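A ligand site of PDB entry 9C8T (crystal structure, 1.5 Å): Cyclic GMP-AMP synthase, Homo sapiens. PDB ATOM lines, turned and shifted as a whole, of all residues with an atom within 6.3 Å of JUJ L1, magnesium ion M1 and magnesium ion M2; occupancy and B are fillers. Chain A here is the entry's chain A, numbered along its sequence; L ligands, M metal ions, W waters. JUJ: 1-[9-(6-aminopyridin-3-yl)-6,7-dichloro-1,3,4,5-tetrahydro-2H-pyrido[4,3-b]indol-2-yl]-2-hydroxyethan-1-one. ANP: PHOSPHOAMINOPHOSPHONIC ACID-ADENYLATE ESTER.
The side-chain hydroxyl (OG1) of Thr 166 is in hydrogen-bond range of a nitrogen (N22) of JUJ L1.
OG1 of Thr 56 is in hydrogen-bond range of N24 of JUJ L1 (3.1 Å).
The backbone carbonyl oxygen (O) of Val 73 is in hydrogen-bond range of a nitrogen (N24) of JUJ L1 (3.2 Å).
O2' of ANP L2 is in hydrogen-bond range of OG of Ser 225 (2.8 Å).
O2B of ANP L2 sits close to N of Ser 58, at 2.9 Å.
The side-chain hydroxyl (OG) of Ser 58 sits at hydrogen-bond distance from an oxygen (O1G) of ANP L2 (2.6 Å).
An oxygen (O2G) of ANP L2 lies within hydrogen-bond range of the side-chain hydroxyl (OG) of Ser 280 (3.0 Å).
Magnesium ion M2 is bound by water W2, 2.0 Å away.
Magnesium ion M2 is bound by the side-chain carboxylate (OE1) of Glu 70, at 2.1 Å.
O2B of ANP L2 binds magnesium ion M2.
OD2 of Asp 72 is bound to magnesium ion M2 (2.1 Å).
An oxygen (O3G) of ANP L2 binds magnesium ion M2 (2.1 Å).
O2A of ANP L2 is bound to magnesium ion M2 (2.1 Å).
O of Asp 72 is in hydrogen-bond range of N of Thr 56, at 3.0 Å.
The backbone carbonyl oxygen (O) of Asp 164 lies within hydrogen-bond range of the backbone NH (N) of Val 73, 2.8 Å away.
The backbone carbonyl oxygen of Phe 71 is in hydrogen-bond range of the backbone NH of Asp 164.
N of Thr 166 sits at hydrogen-bond distance from O of Val 73, at 2.9 Å.
The backbone NH (N) of Arg 221 is in hydrogen-bond range of the backbone carbonyl oxygen (O) of Val 205, at 2.8 Å.
The side-chain hydroxyl (OH) of Tyr 93 sits at hydrogen-bond distance from the side-chain amino group (NZ) of Lys 207.
OG of Ser 223 sits at hydrogen-bond distance from N of Ser 225 (3.3 Å).
O of Leu 54 lies within hydrogen-bond range of N of Met 74, at 2.8 Å.
Water W2 lies within hydrogen-bond range of the side-chain hydroxyl of Ser 58 (2.7 Å) and the backbone carbonyl oxygen of Glu 70 (2.9 Å).
Water W4 lies within hydrogen-bond range of a nitrogen (N10) of JUJ L1 (3.0 Å) and a nitrogen (N6) of ANP L2 (3.3 Å).
Water W3 bridges OG of Ser 150 (2.7 Å) and OD1 of Asp 164 (3.0 Å).
OG of Ser 58 touches magnesium ion M2, at 3.9 Å.
Three residues have an atom within 4 Å of magnesium ion M2: Ser 58, Glu 70 and Asp 72.
Along chain A the residues within 4 Å of magnesium ion M2 span positions 58 to 72.
Met 74 touches JUJ L1 (CG to N24, 3.7 Å).
OG of Ser 150 touches C13 of JUJ L1 (3.7 Å).
CD of Pro 151 touches C07 of JUJ L1 (3.8 Å).
Val 205 touches JUJ L1.
Lys 207 touches JUJ L1.
NH1 of Arg 221 touches CL2 of JUJ L1, at 3.3 Å.
O of Leu 222 touches CL1 of JUJ L1 (3.1 Å).
Ser 223 touches JUJ L1 (CB to CL1, 3.6 Å).
Ser 225 touches JUJ L1.
Hydrophobic or aromatic side chains within 4 Å of JUJ L1: Met 74, Pro 151 and Val 205.
Magnesium ion M1 is bound by the side-chain carboxylate of Asp 72 (2.0 Å), the side-chain carboxylate of Glu 70 (2.0 Å), the side-chain carboxylate of Asp 164 (2.0 Å), an oxygen (O04) of JUJ L1 (2.1 Å), an oxygen (O2A) of ANP L2 (2.1 Å) and an oxygen (O01) of JUJ L1 (2.2 Å).
Magnesium ion M1 has six donor atoms within binding distance.
Of the 26 residues printed, 3 come within 4 Å of magnesium ion M1.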
ATOM      1  N   LEU A  54       7.534 -19.078  -0.708  1.00  0.00           N
ATOM      2  CA  LEU A  54       7.731 -19.303  -2.136  1.00  0.00           C
ATOM      3  C   LEU A  54       6.423 -19.000  -2.819  1.00  0.00           C
ATOM      4  O   LEU A  54       5.422 -19.718  -2.611  1.00  0.00           O
ATOM      5  CB  LEU A  54       8.154 -20.759  -2.373  1.00  0.00           C
ATOM      6  CG  LEU A  54       8.234 -21.323  -3.805  1.00  0.00           C
ATOM      7  CD1 LEU A  54       9.036 -20.428  -4.719  1.00  0.00           C
ATOM      8  CD2 LEU A  54       8.818 -22.770  -3.745  1.00  0.00           C
ATOM      9  N   THR A  56       3.821 -18.922  -5.848  1.00  0.00           N
ATOM     10  CA  THR A  56       3.568 -19.892  -6.925  1.00  0.00           C
ATOM     11  C   THR A  56       2.212 -19.589  -7.557  1.00  0.00           C
ATOM     12  O   THR A  56       1.481 -18.674  -7.126  1.00  0.00           O
ATOM     13  CB  THR A  56       3.539 -21.317  -6.382  1.00  0.00           C
ATOM     14  OG1 THR A  56       2.496 -21.425  -5.416  1.00  0.00           O
ATOM     15  CG2 THR A  56       4.886 -21.714  -5.721  1.00  0.00           C
ATOM     16  N   GLY A  57       1.868 -20.388  -8.598  1.00  0.00           N
ATOM     17  CA  GLY A  57       0.568 -20.302  -9.192  1.00  0.00           C
ATOM     18  C   GLY A  57       0.418 -19.049 -10.064  1.00  0.00           C
ATOM     19  O   GLY A  57       1.355 -18.334 -10.373  1.00  0.00           O
ATOM     20  N   SER A  58      -0.839 -18.881 -10.563  1.00  0.00           N
ATOM     21  CA  SER A  58      -1.063 -18.040 -11.720  1.00  0.00           C
ATOM     22  C   SER A  58      -0.769 -16.576 -11.467  1.00  0.00           C
ATOM     23  O   SER A  58      -0.378 -15.872 -12.391  1.00  0.00           O
ATOM     24  CB  SER A  58      -2.455 -18.186 -12.288  1.00  0.00           C
ATOM     25  OG  SER A  58      -3.412 -17.756 -11.321  1.00  0.00           O
ATOM     26  N   TYR A  59      -0.998 -16.066 -10.269  1.00  0.00           N
ATOM     27  CA  TYR A  59      -0.692 -14.662 -10.039  1.00  0.00           C
ATOM     28  C   TYR A  59       0.793 -14.400 -10.252  1.00  0.00           C
ATOM     29  O   TYR A  59       1.165 -13.451 -10.905  1.00  0.00           O
ATOM     30  CB  TYR A  59      -1.116 -14.289  -8.610  1.00  0.00           C
ATOM     31  CG  TYR A  59      -0.862 -12.819  -8.337  1.00  0.00           C
ATOM     32  CD1 TYR A  59      -1.816 -11.849  -8.677  1.00  0.00           C
ATOM     33  CD2 TYR A  59       0.327 -12.407  -7.734  1.00  0.00           C
ATOM     34  CE1 TYR A  59      -1.576 -10.495  -8.450  1.00  0.00           C
ATOM     35  CE2 TYR A  59       0.567 -11.027  -7.493  1.00  0.00           C
ATOM     36  CZ  TYR A  59      -0.408 -10.116  -7.837  1.00  0.00           C
ATOM     37  OH  TYR A  59      -0.159  -8.768  -7.571  1.00  0.00           O
ATOM     38  N   LYS A  64      -2.871 -15.088 -14.132  1.00  0.00           N
ATOM     39  CA  LYS A  64      -4.144 -14.963 -13.442  1.00  0.00           C
ATOM     40  C   LYS A  64      -5.062 -14.104 -14.304  1.00  0.00           C
ATOM     41  O   LYS A  64      -4.634 -13.069 -14.832  1.00  0.00           O
ATOM     42  CB  LYS A  64      -3.900 -14.307 -12.069  1.00  0.00           C
ATOM     43  CG  LYS A  64      -5.186 -14.095 -11.268  1.00  0.00           C
ATOM     44  CD  LYS A  64      -5.554 -15.423 -10.560  1.00  0.00           C
ATOM     45  CE  LYS A  64      -6.931 -15.394  -9.882  1.00  0.00           C
ATOM     46  NZ  LYS A  64      -8.103 -15.174 -10.817  1.00  0.00           N
ATOM     47  N   GLU A  70      -7.107 -14.806  -6.164  1.00  0.00           N
ATOM     48  CA  GLU A  70      -6.693 -16.143  -5.738  1.00  0.00           C
ATOM     49  C   GLU A  70      -5.182 -16.264  -5.860  1.00  0.00           C
ATOM     50  O   GLU A  70      -4.610 -16.102  -6.949  1.00  0.00           O
ATOM     51  CB  GLU A  70      -7.382 -17.229  -6.538  1.00  0.00           C
ATOM     52  CG  GLU A  70      -7.413 -18.561  -5.751  1.00  0.00           C
ATOM     53  CD  GLU A  70      -6.289 -19.522  -6.112  1.00  0.00           C
ATOM     54  OE1 GLU A  70      -5.477 -19.174  -6.957  1.00  0.00           O
ATOM     55  OE2 GLU A  70      -6.282 -20.648  -5.561  1.00  0.00           O
ATOM     56  N   PHE A  71      -4.537 -16.495  -4.725  1.00  0.00           N
ATOM     57  CA  PHE A  71      -3.095 -16.509  -4.638  1.00  0.00           C
ATOM     58  C   PHE A  71      -2.623 -17.811  -4.012  1.00  0.00           C
ATOM     59  O   PHE A  71      -3.305 -18.358  -3.144  1.00  0.00           O
ATOM     60  CB  PHE A  71      -2.645 -15.415  -3.680  1.00  0.00           C
ATOM     61  CG  PHE A  71      -2.841 -14.031  -4.179  1.00  0.00           C
ATOM     62  CD1 PHE A  71      -4.106 -13.447  -4.186  1.00  0.00           C
ATOM     63  CD2 PHE A  71      -1.735 -13.284  -4.604  1.00  0.00           C
ATOM     64  CE1 PHE A  71      -4.272 -12.098  -4.635  1.00  0.00           C
ATOM     65  CE2 PHE A  71      -1.913 -11.938  -5.041  1.00  0.00           C
ATOM     66  CZ  PHE A  71      -3.215 -11.389  -5.076  1.00  0.00           C
ATOM     67  N   ASP A  72      -1.480 -18.311  -4.472  1.00  0.00           N
ATOM     68  CA  ASP A  72      -0.955 -19.620  -4.057  1.00  0.00           C
ATOM     69  C   ASP A  72       0.434 -19.435  -3.544  1.00  0.00           C
ATOM     70  O   ASP A  72       1.300 -18.912  -4.240  1.00  0.00           O
ATOM     71  CB  ASP A  72      -0.956 -20.557  -5.238  1.00  0.00           C
ATOM     72  CG  ASP A  72      -2.297 -20.704  -5.808  1.00  0.00           C
ATOM     73  OD1 ASP A  72      -3.164 -21.365  -5.185  1.00  0.00           O
ATOM     74  OD2 ASP A  72      -2.522 -20.163  -6.907  1.00  0.00           O
ATOM     75  N   VAL A  73       0.655 -19.795  -2.291  1.00  0.00           N
ATOM     76  CA  VAL A  73       1.956 -19.604  -1.665  1.00  0.00           C
ATOM     77  C   VAL A  73       2.394 -20.880  -1.006  1.00  0.00           C
ATOM     78  O   VAL A  73       1.567 -21.611  -0.455  1.00  0.00           O
ATOM     79  CB  VAL A  73       2.022 -18.431  -0.669  1.00  0.00           C
ATOM     80  CG1 VAL A  73       1.535 -17.105  -1.319  1.00  0.00           C
ATOM     81  CG2 VAL A  73       1.249 -18.764   0.595  1.00  0.00           C
ATOM     82  N   MET A  74       3.666 -21.157  -1.057  1.00  0.00           N
ATOM     83  CA  MET A  74       4.239 -22.321  -0.370  1.00  0.00           C
ATOM     84  C   MET A  74       5.012 -21.770   0.805  1.00  0.00           C
ATOM     85  O   MET A  74       5.721 -20.754   0.677  1.00  0.00           O
ATOM     86  CB  MET A  74       5.172 -23.047  -1.315  1.00  0.00           C
ATOM     87  CG  MET A  74       4.448 -24.069  -2.170  1.00  0.00           C
ATOM     88  SD  MET A  74       5.696 -25.010  -3.126  1.00  0.00           S
ATOM     89  CE  MET A  74       4.681 -26.336  -3.847  1.00  0.00           C
ATOM     90  N   TYR A  93       3.461 -39.956  -5.381  1.00  0.00           N
ATOM     91  CA  TYR A  93       3.243 -39.954  -3.932  1.00  0.00           C
ATOM     92  C   TYR A  93       4.305 -40.786  -3.243  1.00  0.00           C
ATOM     93  O   TYR A  93       4.682 -41.848  -3.730  1.00  0.00           O
ATOM     94  CB  TYR A  93       1.857 -40.464  -3.562  1.00  0.00           C
ATOM     95  CG  TYR A  93       0.731 -39.593  -4.106  1.00  0.00           C
ATOM     96  CD1 TYR A  93       0.226 -39.797  -5.382  1.00  0.00           C
ATOM     97  CD2 TYR A  93       0.226 -38.505  -3.327  1.00  0.00           C
ATOM     98  CE1 TYR A  93      -0.778 -38.992  -5.881  1.00  0.00           C
ATOM     99  CE2 TYR A  93      -0.761 -37.713  -3.821  1.00  0.00           C
ATOM    100  CZ  TYR A  93      -1.260 -37.959  -5.104  1.00  0.00           C
ATOM    101  OH  TYR A  93      -2.239 -37.175  -5.633  1.00  0.00           O
ATOM    102  N   SER A 150      -6.686 -31.308  -1.370  1.00  0.00           N
ATOM    103  CA  SER A 150      -5.719 -30.235  -1.444  1.00  0.00           C
ATOM    104  C   SER A 150      -4.736 -30.334  -0.302  1.00  0.00           C
ATOM    105  O   SER A 150      -5.094 -30.645   0.830  1.00  0.00           O
ATOM    106  CB  SER A 150      -6.420 -28.895  -1.265  1.00  0.00           C
ATOM    107  OG  SER A 150      -5.462 -27.852  -1.259  1.00  0.00           O
ATOM    108  N   PRO A 151      -3.467 -30.022  -0.572  1.00  0.00           N
ATOM    109  CA  PRO A 151      -2.496 -29.911   0.521  1.00  0.00           C
ATOM    110  C   PRO A 151      -2.549 -28.552   1.251  1.00  0.00           C
ATOM    111  O   PRO A 151      -1.791 -28.344   2.231  1.00  0.00           O
ATOM    112  CB  PRO A 151      -1.164 -30.045  -0.205  1.00  0.00           C
ATOM    113  CG  PRO A 151      -1.464 -29.376  -1.579  1.00  0.00           C
ATOM    114  CD  PRO A 151      -2.864 -29.750  -1.890  1.00  0.00           C
ATOM    115  N   ALA A 152      -3.352 -27.611   0.769  1.00  0.00           N
ATOM    116  CA  ALA A 152      -3.286 -26.222   1.207  1.00  0.00           C
ATOM    117  C   ALA A 152      -4.150 -25.995   2.442  1.00  0.00           C
ATOM    118  O   ALA A 152      -5.152 -26.687   2.666  1.00  0.00           O
ATOM    119  CB  ALA A 152      -3.820 -25.333   0.106  1.00  0.00           C
ATOM    120  N   ASP A 164      -4.177 -19.879  -0.890  1.00  0.00           N
ATOM    121  CA  ASP A 164      -3.815 -21.254  -0.573  1.00  0.00           C
ATOM    122  C   ASP A 164      -2.405 -21.235  -0.007  1.00  0.00           C
ATOM    123  O   ASP A 164      -1.440 -20.812  -0.689  1.00  0.00           O
ATOM    124  CB  ASP A 164      -3.813 -22.095  -1.843  1.00  0.00           C
ATOM    125  CG  ASP A 164      -5.214 -22.395  -2.361  1.00  0.00           C
ATOM    126  OD1 ASP A 164      -6.098 -22.726  -1.538  1.00  0.00           O
ATOM    127  OD2 ASP A 164      -5.436 -22.311  -3.573  1.00  0.00           O
ATOM    128  N   ILE A 165      -2.269 -21.643   1.257  1.00  0.00           N
ATOM    129  CA  ILE A 165      -1.001 -21.664   1.952  1.00  0.00           C
ATOM    130  C   ILE A 165      -0.624 -23.117   2.110  1.00  0.00           C
ATOM    131  O   ILE A 165      -1.275 -23.865   2.867  1.00  0.00           O
ATOM    132  CB  ILE A 165      -1.083 -20.988   3.319  1.00  0.00           C
ATOM    133  CG1 ILE A 165      -1.586 -19.566   3.134  1.00  0.00           C
ATOM    134  CG2 ILE A 165       0.273 -21.002   3.954  1.00  0.00           C
ATOM    135  CD1 ILE A 165      -1.659 -18.897   4.467  1.00  0.00           C
ATOM    136  N   THR A 166       0.470 -23.519   1.479  1.00  0.00           N
ATOM    137  CA  THR A 166       0.808 -24.945   1.421  1.00  0.00           C
ATOM    138  C   THR A 166       2.158 -25.181   2.075  1.00  0.00           C
ATOM    139  O   THR A 166       3.175 -24.668   1.613  1.00  0.00           O
ATOM    140  CB  THR A 166       0.786 -25.431  -0.028  1.00  0.00           C
ATOM    141  OG1 THR A 166      -0.541 -25.210  -0.502  1.00  0.00           O
ATOM    142  CG2 THR A 166       1.079 -26.911  -0.094  1.00  0.00           C
ATOM    143  N   VAL A 205       4.455 -31.888  -0.795  1.00  0.00           N
ATOM    144  CA  VAL A 205       3.333 -31.201  -0.197  1.00  0.00           C
ATOM    145  C   VAL A 205       2.440 -32.270   0.421  1.00  0.00           C
ATOM    146  O   VAL A 205       2.399 -33.391  -0.085  1.00  0.00           O
ATOM    147  CB  VAL A 205       2.579 -30.307  -1.226  1.00  0.00           C
ATOM    148  CG1 VAL A 205       3.569 -29.261  -1.818  1.00  0.00           C
ATOM    149  CG2 VAL A 205       1.896 -31.165  -2.365  1.00  0.00           C
ATOM    150  N   LYS A 207      -0.379 -33.697   0.340  1.00  0.00           N
ATOM    151  CA  LYS A 207      -1.525 -34.245  -0.366  1.00  0.00           C
ATOM    152  C   LYS A 207      -1.334 -35.748  -0.413  1.00  0.00           C
ATOM    153  O   LYS A 207      -0.305 -36.237  -0.887  1.00  0.00           O
ATOM    154  CB  LYS A 207      -1.594 -33.703  -1.812  1.00  0.00           C
ATOM    155  CG  LYS A 207      -2.756 -34.290  -2.552  1.00  0.00           C
ATOM    156  CD  LYS A 207      -2.765 -33.781  -3.975  1.00  0.00           C
ATOM    157  CE  LYS A 207      -4.059 -34.241  -4.624  1.00  0.00           C
ATOM    158  NZ  LYS A 207      -4.167 -35.716  -4.579  1.00  0.00           N
ATOM    159  N   ARG A 221       3.204 -35.589  -1.695  1.00  0.00           N
ATOM    160  CA  ARG A 221       3.123 -35.540  -3.141  1.00  0.00           C
ATOM    161  C   ARG A 221       4.225 -34.628  -3.675  1.00  0.00           C
ATOM    162  O   ARG A 221       4.434 -33.535  -3.149  1.00  0.00           O
ATOM    163  CB  ARG A 221       1.794 -35.015  -3.579  1.00  0.00           C
ATOM    164  CG  ARG A 221       1.822 -34.824  -5.059  1.00  0.00           C
ATOM    165  CD  ARG A 221       0.605 -34.941  -5.756  1.00  0.00           C
ATOM    166  NE  ARG A 221       0.968 -34.890  -7.167  1.00  0.00           N
ATOM    167  CZ  ARG A 221       0.089 -35.094  -8.130  1.00  0.00           C
ATOM    168  NH1 ARG A 221      -1.163 -35.431  -7.868  1.00  0.00           N
ATOM    169  NH2 ARG A 221       0.459 -34.894  -9.396  1.00  0.00           N
ATOM    170  N   LEU A 222       4.901 -35.085  -4.717  1.00  0.00           N
ATOM    171  CA  LEU A 222       5.928 -34.295  -5.387  1.00  0.00           C
ATOM    172  C   LEU A 222       5.314 -33.086  -6.068  1.00  0.00           C
ATOM    173  O   LEU A 222       4.295 -33.203  -6.757  1.00  0.00           O
ATOM    174  CB  LEU A 222       6.523 -35.181  -6.467  1.00  0.00           C
ATOM    175  CG  LEU A 222       7.887 -35.774  -6.307  1.00  0.00           C
ATOM    176  CD1 LEU A 222       8.161 -36.570  -7.570  1.00  0.00           C
ATOM    177  CD2 LEU A 222       8.866 -34.570  -6.218  1.00  0.00           C
ATOM    178  N   SER A 223       5.962 -31.931  -5.922  1.00  0.00           N
ATOM    179  CA  SER A 223       5.517 -30.712  -6.587  1.00  0.00           C
ATOM    180  C   SER A 223       6.708 -29.996  -7.223  1.00  0.00           C
ATOM    181  O   SER A 223       7.788 -29.864  -6.618  1.00  0.00           O
ATOM    182  CB  SER A 223       4.877 -29.782  -5.584  1.00  0.00           C
ATOM    183  OG  SER A 223       4.463 -28.599  -6.272  1.00  0.00           O
ATOM    184  N   PHE A 224       6.481 -29.506  -8.444  1.00  0.00           N
ATOM    185  CA  PHE A 224       7.433 -28.646  -9.149  1.00  0.00           C
ATOM    186  C   PHE A 224       6.808 -27.298  -9.484  1.00  0.00           C
ATOM    187  O   PHE A 224       7.127 -26.718 -10.534  1.00  0.00           O
ATOM    188  CB  PHE A 224       7.966 -29.350 -10.394  1.00  0.00           C
ATOM    189  CG  PHE A 224       8.688 -30.621 -10.058  1.00  0.00           C
ATOM    190  CD1 PHE A 224       9.975 -30.549  -9.592  1.00  0.00           C
ATOM    191  CD2 PHE A 224       8.027 -31.853 -10.109  1.00  0.00           C
ATOM    192  CE1 PHE A 224      10.664 -31.668  -9.236  1.00  0.00           C
ATOM    193  CE2 PHE A 224       8.727 -33.019  -9.732  1.00  0.00           C
ATOM    194  CZ  PHE A 224      10.075 -32.880  -9.310  1.00  0.00           C
ATOM    195  N   SER A 225       5.971 -26.785  -8.583  1.00  0.00           N
ATOM    196  CA  SER A 225       5.271 -25.530  -8.895  1.00  0.00           C
ATOM    197  C   SER A 225       6.270 -24.396  -9.122  1.00  0.00           C
ATOM    198  O   SER A 225       5.994 -23.446  -9.877  1.00  0.00           O
ATOM    199  CB  SER A 225       4.357 -25.216  -7.696  1.00  0.00           C
ATOM    200  OG  SER A 225       3.416 -24.217  -8.024  1.00  0.00           O
ATOM    201  N   SER A 280      -7.804 -25.805 -13.871  1.00  0.00           N
ATOM    202  CA  SER A 280      -6.880 -25.077 -14.704  1.00  0.00           C
ATOM    203  C   SER A 280      -5.537 -25.787 -14.837  1.00  0.00           C
ATOM    204  O   SER A 280      -4.824 -25.516 -15.796  1.00  0.00           O
ATOM    205  CB  SER A 280      -6.711 -23.651 -14.159  1.00  0.00           C
ATOM    206  OG  SER A 280      -6.150 -23.690 -12.861  1.00  0.00           O
HETATM  207  C13 JUJ L   1      -5.638 -27.357  -4.958  1.00  0.00           C
HETATM  208  C20 JUJ L   1       0.186 -26.866  -4.685  1.00  0.00           C
HETATM  209  C21 JUJ L   1      -0.423 -26.259  -3.594  1.00  0.00           C
HETATM  210  C26 JUJ L   1       1.143 -26.048  -5.356  1.00  0.00           C
HETATM  211  O01 JUJ L   1      -6.742 -23.432  -5.897  1.00  0.00           O
HETATM  212  C02 JUJ L   1      -6.526 -24.797  -5.648  1.00  0.00           C
HETATM  213  C03 JUJ L   1      -5.049 -25.036  -5.376  1.00  0.00           C
HETATM  214  O04 JUJ L   1      -4.246 -24.152  -5.390  1.00  0.00           O
HETATM  215  N05 JUJ L   1      -4.683 -26.239  -5.126  1.00  0.00           N
HETATM  216  C06 JUJ L   1      -3.299 -26.556  -4.762  1.00  0.00           C
HETATM  217  C07 JUJ L   1      -2.883 -27.973  -5.220  1.00  0.00           C
HETATM  218  C08 JUJ L   1      -1.560 -28.566  -5.330  1.00  0.00           C
HETATM  219  C09 JUJ L   1      -1.831 -29.901  -5.838  1.00  0.00           C
HETATM  220  N10 JUJ L   1      -3.207 -30.039  -5.963  1.00  0.00           N
HETATM  221  C11 JUJ L   1      -3.814 -28.867  -5.593  1.00  0.00           C
HETATM  222  C12 JUJ L   1      -5.271 -28.653  -5.635  1.00  0.00           C
HETATM  223  C14 JUJ L   1      -0.823 -30.747  -6.113  1.00  0.00           C
HETATM  224 CL2  JUJ L   1      -1.225 -32.350  -6.746  1.00  0.00          CL
HETATM  225  C16 JUJ L   1       0.455 -30.359  -5.917  1.00  0.00           C
HETATM  226 CL1  JUJ L   1       1.777 -31.396  -6.334  1.00  0.00          CL
HETATM  227  C18 JUJ L   1       0.771 -29.083  -5.450  1.00  0.00           C
HETATM  228  C19 JUJ L   1      -0.194 -28.206  -5.159  1.00  0.00           C
HETATM  229  N22 JUJ L   1      -0.135 -25.037  -3.087  1.00  0.00           N
HETATM  230  C23 JUJ L   1       0.783 -24.239  -3.752  1.00  0.00           C
HETATM  231  N24 JUJ L   1       1.032 -23.000  -3.244  1.00  0.00           N
HETATM  232  C25 JUJ L   1       1.439 -24.758  -4.903  1.00  0.00           C
HETATM  233  PG  ANP L   2      -5.666 -20.311 -11.237  1.00  0.00           P
HETATM  234  O1G ANP L   2      -5.614 -18.982 -11.956  1.00  0.00           O
HETATM  235  O2G ANP L   2      -6.970 -21.100 -11.675  1.00  0.00           O
HETATM  236  O3G ANP L   2      -5.615 -20.148  -9.741  1.00  0.00           O
HETATM  237  PB  ANP L   2      -3.226 -21.793 -10.752  1.00  0.00           P
HETATM  238  O1B ANP L   2      -2.079 -22.401 -11.489  1.00  0.00           O
HETATM  239  O2B ANP L   2      -2.807 -20.786  -9.686  1.00  0.00           O
HETATM  240  N3B ANP L   2      -4.282 -21.109 -11.776  1.00  0.00           N
HETATM  241  PA  ANP L   2      -4.367 -23.261  -8.523  1.00  0.00           P
HETATM  242  O1A ANP L   2      -5.523 -24.205  -8.604  1.00  0.00           O
HETATM  243  O2A ANP L   2      -4.528 -22.054  -7.616  1.00  0.00           O
HETATM  244  O3A ANP L   2      -3.991 -23.008 -10.041  1.00  0.00           O
HETATM  245  O5' ANP L   2      -3.144 -24.194  -8.051  1.00  0.00           O
HETATM  246  C5' ANP L   2      -1.909 -23.594  -7.657  1.00  0.00           C
HETATM  247  C4' ANP L   2      -0.759 -24.500  -8.067  1.00  0.00           C
HETATM  248  O4' ANP L   2      -0.941 -25.821  -7.515  1.00  0.00           O
HETATM  249  C3' ANP L   2      -0.658 -24.766  -9.572  1.00  0.00           C
HETATM  250  O3' ANP L   2      -0.062 -23.700 -10.289  1.00  0.00           O
HETATM  251  C2' ANP L   2       0.166 -26.046  -9.604  1.00  0.00           C
HETATM  252  O2' ANP L   2       1.552 -25.779  -9.471  1.00  0.00           O
HETATM  253  C1' ANP L   2      -0.337 -26.785  -8.359  1.00  0.00           C
HETATM  254  N9  ANP L   2      -1.332 -27.781  -8.692  1.00  0.00           N
HETATM  255  C8  ANP L   2      -2.701 -27.634  -8.785  1.00  0.00           C
HETATM  256  N7  ANP L   2      -3.334 -28.717  -9.162  1.00  0.00           N
HETATM  257  C5  ANP L   2      -2.320 -29.617  -9.374  1.00  0.00           C
HETATM  258  C6  ANP L   2      -2.338 -30.967  -9.796  1.00  0.00           C
HETATM  259  N6  ANP L   2      -3.453 -31.608 -10.130  1.00  0.00           N
HETATM  260  N1  ANP L   2      -1.153 -31.581  -9.920  1.00  0.00           N
HETATM  261  C2  ANP L   2      -0.032 -30.932  -9.586  1.00  0.00           C
HETATM  262  N3  ANP L   2       0.113 -29.679  -9.146  1.00  0.00           N
HETATM  263  C4  ANP L   2      -1.085 -29.068  -9.092  1.00  0.00           C
HETATM  264 MG    MG M   1      -4.965 -22.201  -5.560  1.00  0.00          MG
HETATM  265 MG    MG M   2      -4.116 -20.055  -8.251  1.00  0.00          MG
HETATM  266  O   HOH W   1      -8.729 -22.852  -7.349  1.00  0.00           O
HETATM  267  O   HOH W   2      -3.532 -18.170  -8.663  1.00  0.00           O
HETATM  268  O   HOH W   3      -6.592 -25.604  -2.222  1.00  0.00           O
HETATM  269  O   HOH W   4      -5.001 -32.089  -7.221  1.00  0.00           O
